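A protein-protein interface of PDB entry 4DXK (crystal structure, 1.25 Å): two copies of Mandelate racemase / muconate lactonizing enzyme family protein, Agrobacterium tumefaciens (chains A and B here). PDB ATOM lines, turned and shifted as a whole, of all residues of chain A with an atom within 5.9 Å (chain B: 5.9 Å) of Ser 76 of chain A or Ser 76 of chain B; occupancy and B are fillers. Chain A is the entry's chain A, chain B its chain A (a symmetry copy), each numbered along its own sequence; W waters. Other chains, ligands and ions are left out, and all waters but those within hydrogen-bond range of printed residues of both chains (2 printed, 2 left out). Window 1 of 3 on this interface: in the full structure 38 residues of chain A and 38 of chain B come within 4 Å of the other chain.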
ATOM      1  N   GLY A  73     -18.042  12.440  -2.931  1.00  0.00           N
ATOM      2  CA  GLY A  73     -18.718  11.958  -4.126  1.00  0.00           C
ATOM      3  C   GLY A  73     -17.819  11.362  -5.192  1.00  0.00           C
ATOM      4  O   GLY A  73     -18.288  11.022  -6.281  1.00  0.00           O
ATOM      5  N   PHE A  74     -16.541  11.211  -4.880  1.00  0.00           N
ATOM      6  CA  PHE A  74     -15.556  10.619  -5.778  1.00  0.00           C
ATOM      7  C   PHE A  74     -15.716   9.084  -5.792  1.00  0.00           C
ATOM      8  O   PHE A  74     -16.433   8.513  -4.970  1.00  0.00           O
ATOM      9  CB  PHE A  74     -14.154  11.024  -5.297  1.00  0.00           C
ATOM     10  CG  PHE A  74     -13.869  10.578  -3.906  1.00  0.00           C
ATOM     11  CD1 PHE A  74     -13.354   9.314  -3.655  1.00  0.00           C
ATOM     12  CD2 PHE A  74     -14.179  11.396  -2.824  1.00  0.00           C
ATOM     13  CE1 PHE A  74     -13.131   8.876  -2.363  1.00  0.00           C
ATOM     14  CE2 PHE A  74     -13.954  10.961  -1.533  1.00  0.00           C
ATOM     15  CZ  PHE A  74     -13.436   9.704  -1.294  1.00  0.00           C
ATOM     16  N   ARG A  75     -15.021   8.425  -6.721  1.00  0.00           N
ATOM     17  CA  ARG A  75     -15.040   6.965  -6.847  1.00  0.00           C
ATOM     18  C   ARG A  75     -16.481   6.456  -6.827  1.00  0.00           C
ATOM     19  O   ARG A  75     -16.832   5.536  -6.087  1.00  0.00           O
ATOM     20  CB  ARG A  75     -14.191   6.302  -5.756  1.00  0.00           C
ATOM     21  CG  ARG A  75     -13.930   4.804  -5.976  1.00  0.00           C
ATOM     22  CD  ARG A  75     -14.153   4.052  -4.684  1.00  0.00           C
ATOM     23  NE  ARG A  75     -13.899   2.610  -4.772  1.00  0.00           N
ATOM     24  CZ  ARG A  75     -14.842   1.690  -4.964  1.00  0.00           C
ATOM     25  NH1 ARG A  75     -16.113   2.051  -5.121  1.00  0.00           N
ATOM     26  NH2 ARG A  75     -14.507   0.405  -4.995  1.00  0.00           N
ATOM     27  N   SER A  76     -17.312   7.072  -7.660  1.00  0.00           N
ATOM     28  CA  SER A  76     -18.723   6.744  -7.687  1.00  0.00           C
ATOM     29  C   SER A  76     -19.302   7.117  -9.032  1.00  0.00           C
ATOM     30  O   SER A  76     -18.624   7.706  -9.880  1.00  0.00           O
ATOM     31  CB  SER A  76     -19.464   7.493  -6.588  1.00  0.00           C
ATOM     32  OG  SER A  76     -19.808   8.795  -7.018  1.00  0.00           O
ATOM     33  N   SER A  77     -20.573   6.775  -9.212  1.00  0.00           N
ATOM     34  CA  SER A  77     -21.340   7.171 -10.391  1.00  0.00           C
ATOM     35  C   SER A  77     -22.417   8.196 -10.013  1.00  0.00           C
ATOM     36  O   SER A  77     -23.437   8.304 -10.687  1.00  0.00           O
ATOM     37  CB  SER A  77     -21.952   5.938 -11.053  1.00  0.00           C
ATOM     38  OG  SER A  77     -22.612   5.138 -10.088  1.00  0.00           O
ATOM     39  N   GLY A  78     -22.169   8.951  -8.945  1.00  0.00           N
ATOM     40  CA  GLY A  78     -23.102   9.971  -8.480  1.00  0.00           C
ATOM     41  C   GLY A  78     -23.153  11.212  -9.355  1.00  0.00           C
ATOM     42  O   GLY A  78     -22.457  11.327 -10.368  1.00  0.00           O
ATOM     43  N   ALA A  79     -23.971  12.171  -8.932  1.00  0.00           N
ATOM     44  CA  ALA A  79     -24.314  13.308  -9.788  1.00  0.00           C
ATOM     45  C   ALA A  79     -23.095  14.126 -10.171  1.00  0.00           C
ATOM     46  O   ALA A  79     -22.963  14.561 -11.323  1.00  0.00           O
ATOM     47  CB  ALA A  79     -25.359  14.186  -9.121  1.00  0.00           C
ATOM     48  N   GLU A  80     -22.212  14.359  -9.212  1.00  0.00           N
ATOM     49  CA  GLU A  80     -21.000  15.127  -9.474  1.00  0.00           C
ATOM     50  C   GLU A  80     -20.157  14.446 -10.555  1.00  0.00           C
ATOM     51  O   GLU A  80     -19.680  15.089 -11.498  1.00  0.00           O
ATOM     52  CB  GLU A  80     -20.169  15.299  -8.194  1.00  0.00           C
ATOM     53  CG  GLU A  80     -20.848  16.096  -7.078  1.00  0.00           C
ATOM     54  CD  GLU A  80     -21.597  15.269  -6.047  1.00  0.00           C
ATOM     55  OE1 GLU A  80     -22.011  14.124  -6.315  1.00  0.00           O
ATOM     56  OE2 GLU A  80     -21.778  15.801  -4.935  1.00  0.00           O
ATOM     57  N   VAL A  81     -19.958  13.139 -10.415  1.00  0.00           N
ATOM     58  CA  VAL A  81     -19.178  12.408 -11.395  1.00  0.00           C
ATOM     59  C   VAL A  81     -19.856  12.417 -12.763  1.00  0.00           C
ATOM     60  O   VAL A  81     -19.178  12.578 -13.785  1.00  0.00           O
ATOM     61  CB  VAL A  81     -18.870  10.985 -10.919  1.00  0.00           C
ATOM     62  CG1 VAL A  81     -18.258  10.159 -12.049  1.00  0.00           C
ATOM     63  CG2 VAL A  81     -17.928  11.057  -9.714  1.00  0.00           C
ATOM     64  N   THR A 269     -21.847   0.691 -13.227  1.00  0.00           N
ATOM     65  CA  THR A 269     -22.171   1.452 -12.013  1.00  0.00           C
ATOM     66  C   THR A 269     -20.957   1.954 -11.235  1.00  0.00           C
ATOM     67  O   THR A 269     -21.127   2.726 -10.293  1.00  0.00           O
ATOM     68  CB  THR A 269     -23.085   0.663 -11.032  1.00  0.00           C
ATOM     69  OG1 THR A 269     -22.351  -0.405 -10.414  1.00  0.00           O
ATOM     70  CG2 THR A 269     -24.301   0.098 -11.750  1.00  0.00           C
ATOM     71  N   LEU A 270     -19.753   1.525 -11.617  1.00  0.00           N
ATOM     72  CA  LEU A 270     -18.525   1.893 -10.919  1.00  0.00           C
ATOM     73  C   LEU A 270     -17.882   3.118 -11.547  1.00  0.00           C
ATOM     74  O   LEU A 270     -17.886   3.272 -12.777  1.00  0.00           O
ATOM     75  CB  LEU A 270     -17.516   0.734 -10.951  1.00  0.00           C
ATOM     76  CG  LEU A 270     -17.882  -0.480 -10.098  1.00  0.00           C
ATOM     77  CD1 LEU A 270     -16.921  -1.625 -10.383  1.00  0.00           C
ATOM     78  CD2 LEU A 270     -17.887  -0.149  -8.606  1.00  0.00           C
ATOM     79  N   GLY A 271     -17.295   3.973 -10.717  1.00  0.00           N
ATOM     80  CA  GLY A 271     -16.649   5.179 -11.206  1.00  0.00           C
ATOM     81  C   GLY A 271     -15.193   5.336 -10.806  1.00  0.00           C
ATOM     82  O   GLY A 271     -14.814   5.038  -9.671  1.00  0.00           O
ATOM     83  N   SER A 272     -14.408   5.805 -11.773  1.00  0.00           N
ATOM     84  CA  SER A 272     -12.987   6.162 -11.631  1.00  0.00           C
ATOM     85  C   SER A 272     -12.094   4.933 -11.715  1.00  0.00           C
ATOM     86  O   SER A 272     -12.494   3.801 -11.404  1.00  0.00           O
ATOM     87  CB  SER A 272     -12.678   6.942 -10.342  1.00  0.00           C
ATOM     88  OG  SER A 272     -12.407   6.062  -9.256  1.00  0.00           O
ATOM     89  N   TRP A 294     -20.622   7.994 -16.749  1.00  0.00           N
ATOM     90  CA  TRP A 294     -20.860   7.667 -15.345  1.00  0.00           C
ATOM     91  C   TRP A 294     -19.558   7.395 -14.587  1.00  0.00           C
ATOM     92  O   TRP A 294     -19.600   7.255 -13.368  1.00  0.00           O
ATOM     93  CB  TRP A 294     -21.763   6.430 -15.211  1.00  0.00           C
ATOM     94  CG  TRP A 294     -23.151   6.592 -15.761  1.00  0.00           C
ATOM     95  CD1 TRP A 294     -23.770   7.764 -16.095  1.00  0.00           C
ATOM     96  CD2 TRP A 294     -24.081   5.541 -16.079  1.00  0.00           C
ATOM     97  NE1 TRP A 294     -25.028   7.507 -16.582  1.00  0.00           N
ATOM     98  CE2 TRP A 294     -25.248   6.154 -16.578  1.00  0.00           C
ATOM     99  CE3 TRP A 294     -24.056   4.146 -15.954  1.00  0.00           C
ATOM    100  CZ2 TRP A 294     -26.370   5.422 -16.971  1.00  0.00           C
ATOM    101  CZ3 TRP A 294     -25.167   3.419 -16.353  1.00  0.00           C
ATOM    102  CH2 TRP A 294     -26.310   4.058 -16.846  1.00  0.00           C
ATOM    103  N   CYS A 295     -18.420   7.295 -15.289  1.00  0.00           N
ATOM    104  CA  CYS A 295     -17.195   6.770 -14.674  1.00  0.00           C
ATOM    105  C   CYS A 295     -16.063   7.769 -14.570  1.00  0.00           C
ATOM    106  O   CYS A 295     -14.993   7.412 -14.076  1.00  0.00           O
ATOM    107  CB  CYS A 295     -16.689   5.537 -15.441  1.00  0.00           C
ATOM    108  SG  CYS A 295     -15.900   5.912 -17.020  1.00  0.00           S
ATOM    109  N   GLY A 296     -16.272   8.984 -15.070  1.00  0.00           N
ATOM    110  CA  GLY A 296     -15.207   9.978 -15.122  1.00  0.00           C
ATOM    111  C   GLY A 296     -14.788  10.379 -16.531  1.00  0.00           C
ATOM    112  O   GLY A 296     -13.711  10.953 -16.727  1.00  0.00           O
ATOM    113  N   GLY B  73     -24.445   6.093  -7.906  1.00  0.00           N
ATOM    114  CA  GLY B  73     -24.126   7.049  -6.856  1.00  0.00           C
ATOM    115  C   GLY B  73     -24.168   6.507  -5.441  1.00  0.00           C
ATOM    116  O   GLY B  73     -24.013   7.265  -4.480  1.00  0.00           O
ATOM    117  N   PHE B  74     -24.349   5.201  -5.306  1.00  0.00           N
ATOM    118  CA  PHE B  74     -24.376   4.519  -4.017  1.00  0.00           C
ATOM    119  C   PHE B  74     -22.937   4.356  -3.482  1.00  0.00           C
ATOM    120  O   PHE B  74     -21.964   4.586  -4.200  1.00  0.00           O
ATOM    121  CB  PHE B  74     -25.055   3.153  -4.203  1.00  0.00           C
ATOM    122  CG  PHE B  74     -24.354   2.291  -5.192  1.00  0.00           C
ATOM    123  CD1 PHE B  74     -23.302   1.472  -4.805  1.00  0.00           C
ATOM    124  CD2 PHE B  74     -24.696   2.339  -6.540  1.00  0.00           C
ATOM    125  CE1 PHE B  74     -22.616   0.703  -5.726  1.00  0.00           C
ATOM    126  CE2 PHE B  74     -24.014   1.569  -7.462  1.00  0.00           C
ATOM    127  CZ  PHE B  74     -22.972   0.754  -7.065  1.00  0.00           C
ATOM    128  N   ARG B  75     -22.819   3.936  -2.221  1.00  0.00           N
ATOM    129  CA  ARG B  75     -21.525   3.700  -1.575  1.00  0.00           C
ATOM    130  C   ARG B  75     -20.600   4.895  -1.806  1.00  0.00           C
ATOM    131  O   ARG B  75     -19.449   4.753  -2.220  1.00  0.00           O
ATOM    132  CB  ARG B  75     -20.890   2.392  -2.061  1.00  0.00           C
ATOM    133  CG  ARG B  75     -19.676   1.932  -1.241  1.00  0.00           C
ATOM    134  CD  ARG B  75     -18.564   1.503  -2.171  1.00  0.00           C
ATOM    135  NE  ARG B  75     -17.362   1.010  -1.488  1.00  0.00           N
ATOM    136  CZ  ARG B  75     -16.282   1.748  -1.241  1.00  0.00           C
ATOM    137  NH1 ARG B  75     -16.249   3.032  -1.589  1.00  0.00           N
ATOM    138  NH2 ARG B  75     -15.232   1.194  -0.646  1.00  0.00           N
ATOM    139  N   SER B  76     -21.126   6.082  -1.526  1.00  0.00           N
ATOM    140  CA  SER B  76     -20.389   7.305  -1.774  1.00  0.00           C
ATOM    141  C   SER B  76     -20.917   8.403  -0.880  1.00  0.00           C
ATOM    142  O   SER B  76     -21.902   8.222  -0.157  1.00  0.00           O
ATOM    143  CB  SER B  76     -20.526   7.723  -3.230  1.00  0.00           C
ATOM    144  OG  SER B  76     -21.717   8.460  -3.426  1.00  0.00           O
ATOM    145  N   SER B  77     -20.253   9.552  -0.947  1.00  0.00           N
ATOM    146  CA  SER B  77     -20.696  10.763  -0.262  1.00  0.00           C
ATOM    147  C   SER B  77     -21.179  11.810  -1.275  1.00  0.00           C
ATOM    148  O   SER B  77     -21.140  13.005  -1.001  1.00  0.00           O
ATOM    149  CB  SER B  77     -19.568  11.311   0.610  1.00  0.00           C
ATOM    150  OG  SER B  77     -18.365  11.389  -0.133  1.00  0.00           O
ATOM    151  N   GLY B  78     -21.645  11.344  -2.433  1.00  0.00           N
ATOM    152  CA  GLY B  78     -22.143  12.227  -3.481  1.00  0.00           C
ATOM    153  C   GLY B  78     -23.496  12.849  -3.177  1.00  0.00           C
ATOM    154  O   GLY B  78     -24.103  12.616  -2.129  1.00  0.00           O
ATOM    155  N   ALA B  79     -23.988  13.631  -4.135  1.00  0.00           N
ATOM    156  CA  ALA B  79     -25.148  14.490  -3.892  1.00  0.00           C
ATOM    157  C   ALA B  79     -26.383  13.693  -3.514  1.00  0.00           C
ATOM    158  O   ALA B  79     -27.139  14.088  -2.618  1.00  0.00           O
ATOM    159  CB  ALA B  79     -25.427  15.370  -5.097  1.00  0.00           C
ATOM    160  N   GLU B  80     -26.608  12.586  -4.205  1.00  0.00           N
ATOM    161  CA  GLU B  80     -27.761  11.741  -3.920  1.00  0.00           C
ATOM    162  C   GLU B  80     -27.713  11.237  -2.475  1.00  0.00           C
ATOM    163  O   GLU B  80     -28.709  11.284  -1.744  1.00  0.00           O
ATOM    164  CB  GLU B  80     -27.825  10.549  -4.887  1.00  0.00           C
ATOM    165  CG  GLU B  80     -28.022  10.916  -6.360  1.00  0.00           C
ATOM    166  CD  GLU B  80     -26.748  11.045  -7.177  1.00  0.00           C
ATOM    167  OE1 GLU B  80     -25.653  11.285  -6.631  1.00  0.00           O
ATOM    168  OE2 GLU B  80     -26.863  10.907  -8.409  1.00  0.00           O
ATOM    169  N   VAL B  81     -26.552  10.738  -2.061  1.00  0.00           N
ATOM    170  CA  VAL B  81     -26.410  10.244  -0.705  1.00  0.00           C
ATOM    171  C   VAL B  81     -26.583  11.365   0.316  1.00  0.00           C
ATOM    172  O   VAL B  81     -27.228  11.161   1.351  1.00  0.00           O
ATOM    173  CB  VAL B  81     -25.086   9.498  -0.515  1.00  0.00           C
ATOM    174  CG1 VAL B  81     -24.845   9.192   0.962  1.00  0.00           C
ATOM    175  CG2 VAL B  81     -25.114   8.214  -1.349  1.00  0.00           C
ATOM    176  N   THR B 269     -15.450  10.948   4.506  1.00  0.00           N
ATOM    177  CA  THR B 269     -15.700  10.949   3.058  1.00  0.00           C
ATOM    178  C   THR B 269     -16.324   9.663   2.521  1.00  0.00           C
ATOM    179  O   THR B 269     -16.707   9.626   1.353  1.00  0.00           O
ATOM    180  CB  THR B 269     -14.422  11.254   2.226  1.00  0.00           C
ATOM    181  OG1 THR B 269     -13.515  10.141   2.277  1.00  0.00           O
ATOM    182  CG2 THR B 269     -13.722  12.506   2.733  1.00  0.00           C
ATOM    183  N   LEU B 270     -16.423   8.625   3.353  1.00  0.00           N
ATOM    184  CA  LEU B 270     -16.953   7.329   2.939  1.00  0.00           C
ATOM    185  C   LEU B 270     -18.442   7.228   3.223  1.00  0.00           C
ATOM    186  O   LEU B 270     -18.922   7.718   4.255  1.00  0.00           O
ATOM    187  CB  LEU B 270     -16.232   6.190   3.677  1.00  0.00           C
ATOM    188  CG  LEU B 270     -14.778   5.958   3.267  1.00  0.00           C
ATOM    189  CD1 LEU B 270     -14.124   4.958   4.210  1.00  0.00           C
ATOM    190  CD2 LEU B 270     -14.661   5.479   1.821  1.00  0.00           C
ATOM    191  N   GLY B 271     -19.173   6.564   2.334  1.00  0.00           N
ATOM    192  CA  GLY B 271     -20.607   6.405   2.502  1.00  0.00           C
ATOM    193  C   GLY B 271     -21.101   4.969   2.494  1.00  0.00           C
ATOM    194  O   GLY B 271     -20.635   4.146   1.703  1.00  0.00           O
ATOM    195  N   SER B 272     -22.044   4.711   3.396  1.00  0.00           N
ATOM    196  CA  SER B 272     -22.779   3.443   3.534  1.00  0.00           C
ATOM    197  C   SER B 272     -21.972   2.414   4.311  1.00  0.00           C
ATOM    198  O   SER B 272     -20.733   2.431   4.342  1.00  0.00           O
ATOM    199  CB  SER B 272     -23.226   2.847   2.189  1.00  0.00           C
ATOM    200  OG  SER B 272     -22.212   2.020   1.626  1.00  0.00           O
ATOM    201  N   TRP B 294     -23.439  12.630   5.271  1.00  0.00           N
ATOM    202  CA  TRP B 294     -22.677  12.259   4.080  1.00  0.00           C
ATOM    203  C   TRP B 294     -22.633  10.744   3.871  1.00  0.00           C
ATOM    204  O   TRP B 294     -22.154  10.303   2.830  1.00  0.00           O
ATOM    205  CB  TRP B 294     -21.231  12.776   4.168  1.00  0.00           C
ATOM    206  CG  TRP B 294     -21.091  14.271   4.210  1.00  0.00           C
ATOM    207  CD1 TRP B 294     -22.050  15.195   3.901  1.00  0.00           C
ATOM    208  CD2 TRP B 294     -19.931  15.017   4.621  1.00  0.00           C
ATOM    209  NE1 TRP B 294     -21.553  16.463   4.077  1.00  0.00           N
ATOM    210  CE2 TRP B 294     -20.255  16.384   4.513  1.00  0.00           C
ATOM    211  CE3 TRP B 294     -18.639  14.663   5.033  1.00  0.00           C
ATOM    212  CZ2 TRP B 294     -19.344  17.398   4.820  1.00  0.00           C
ATOM    213  CZ3 TRP B 294     -17.739  15.669   5.346  1.00  0.00           C
ATOM    214  CH2 TRP B 294     -18.092  17.018   5.230  1.00  0.00           C
ATOM    215  N   CYS B 295     -23.099   9.952   4.847  1.00  0.00           N
ATOM    216  CA  CYS B 295     -22.841   8.507   4.836  1.00  0.00           C
ATOM    217  C   CYS B 295     -24.077   7.646   4.691  1.00  0.00           C
ATOM    218  O   CYS B 295     -23.956   6.420   4.682  1.00  0.00           O
ATOM    219  CB  CYS B 295     -22.097   8.080   6.112  1.00  0.00           C
ATOM    220  SG  CYS B 295     -23.126   8.024   7.593  1.00  0.00           S
ATOM    221  N   GLY B 296     -25.251   8.268   4.626  1.00  0.00           N
ATOM    222  CA  GLY B 296     -26.504   7.525   4.602  1.00  0.00           C
ATOM    223  C   GLY B 296     -27.394   7.748   5.819  1.00  0.00           C
ATOM    224  O   GLY B 296     -28.310   6.961   6.081  1.00  0.00           O
HETATM  225  O   HOH W   1     -21.626   5.029  -6.977  1.00  0.00           O
HETATM  226  O   HOH W   2     -17.715   9.324  -2.577  1.00  0.00           O
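Gly 73 of chain A touches Gly 78 of chain B, and with the chains exchanged Gly 78 of chain A touches Gly 73 of chain B.
Arg 75 of chain A touches its own counterpart, Arg 75 of chain B.
Gly 78 of chain A touches Glu 80 of chain B, and with the chains exchanged Glu 80 of chain A touches Gly 78 of chain B.
Ala 79 of chain A touches Glu 80 of chain B, and with the chains exchanged Glu 80 of chain A touches Ala 79 of chain B.
Positions printed for both chains: 73, 74, 75, 76, 77, 78, 79, 80, 81, 269, 270, 271, 272, 294, 295 and 296.
Of the 16 printed residues of chain B, 9 touch a printed residue of chain A.
Hydrophobic or aromatic side chains of chain B that line the printed part of chain A: Phe 74 and Ala 79.
Along chain B the printed residues that touch a printed residue of chain A span positions 73 to 269.
Hydrophobic or aromatic side chains of chain A that line the printed part of chain B: Phe 74 and Ala 79.
The side-chain hydroxyl (OG) of Ser 76 of chain A is in hydrogen-bond range of the backbone carbonyl oxygen (O) of Gly 73 of chain A.
The side-chain hydroxyl of Ser 76 of chain A is in hydrogen-bond range of the backbone NH of Gly 78 of chain A, 3.1 Å away.
The side-chain hydroxyl (OG) of Ser 77 of chain A is in hydrogen-bond range of the backbone carbonyl oxygen (O) of Thr 269 of chain A, 2.8 Å away.
The backbone carbonyl oxygen (O) of Gly 73 of chain B is in hydrogen-bond range of the side-chain hydroxyl (OG) of Ser 76 of chain B (2.8 Å).
N of Gly 78 of chain B lies within hydrogen-bond range of OG of Ser 76 of chain B (3.1 Å).
The side-chain hydroxyl (OG) of Ser 77 of chain B is in hydrogen-bond range of the backbone carbonyl oxygen (O) of Thr 269 of chain B (2.8 Å).
CA of Gly 73 of chain A touches N of Gly 78 of chain B, at 3.4 Å.
OG1 of Thr 269 of chain B touches CZ of Phe 74 of chain A (3.6 Å).
NH1 of Arg 75 of chain B touches NH1 of Arg 75 of chain A, 3.7 Å away.
Ser 76 of chain A touches Ser 76 of chain B.
Gly 73 of chain B touches Gly 78 of chain A (CA to N, 3.4 Å).
Gly 78 of chain A touches Glu 80 of chain B.
CA of Gly 78 of chain B touches OE1 of Glu 80 of chain A, at 3.4 Å.
CZ of Phe 74 of chain B touches OG1 of Thr 269 of chain A, at 3.6 Å.
The backbone NH (N) of Gly 73 of chain A sits at hydrogen-bond distance from the side-chain hydroxyl (OG) of Ser 77 of chain B, 3.0 Å away.
The side-chain hydroxyl of Ser 77 of chain A sits at hydrogen-bond distance from the backbone NH of Gly 73 of chain B.
OE1 of Glu 80 of chain B lies within hydrogen-bond range of N of Ala 79 of chain A, at 3.0 Å.
N of Ala 79 of chain B lies within hydrogen-bond range of OE1 of Glu 80 of chain A.
Water W2 lies within hydrogen-bond range of O of Phe 74 of chain A, N of Ser 77 of chain B and N of Gly 73 of chain A.
Water W1 lies within hydrogen-bond range of the backbone carbonyl oxygen (O) of Phe 74 of chain B (2.8 Å), the backbone NH (N) of Ser 77 of chain A (3.0 Å) and the backbone NH (N) of Gly 73 of chain B (3.2 Å).
Of chain B, only Ser 76 comes within 4 Å of Ser 76 of chain A.
Of chain A, only Ser 76 (3.5 Å) comes within 4 Å of Ser 76 of chain B.
Printed residues of chain B within 4 Å of Arg 75 of chain A: Arg 75.
Of the printed residues of chain B, Gly 73 of chain A touches Ser 77 (3.0 Å) and Gly 78 (3.4 Å).
Gly 296 of chain B touches none of the printed residues of chain A.
Trp 294 of chain B touches none of the printed residues of chain A.
The nearest residue of chain B that does not touch Ser 76 of chain A is Phe 74 of chain B (4.5 Å).
The nearest printed residue of chain A that does not touch Thr 269 of chain B is Gly 73 of chain A (5.3 Å).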
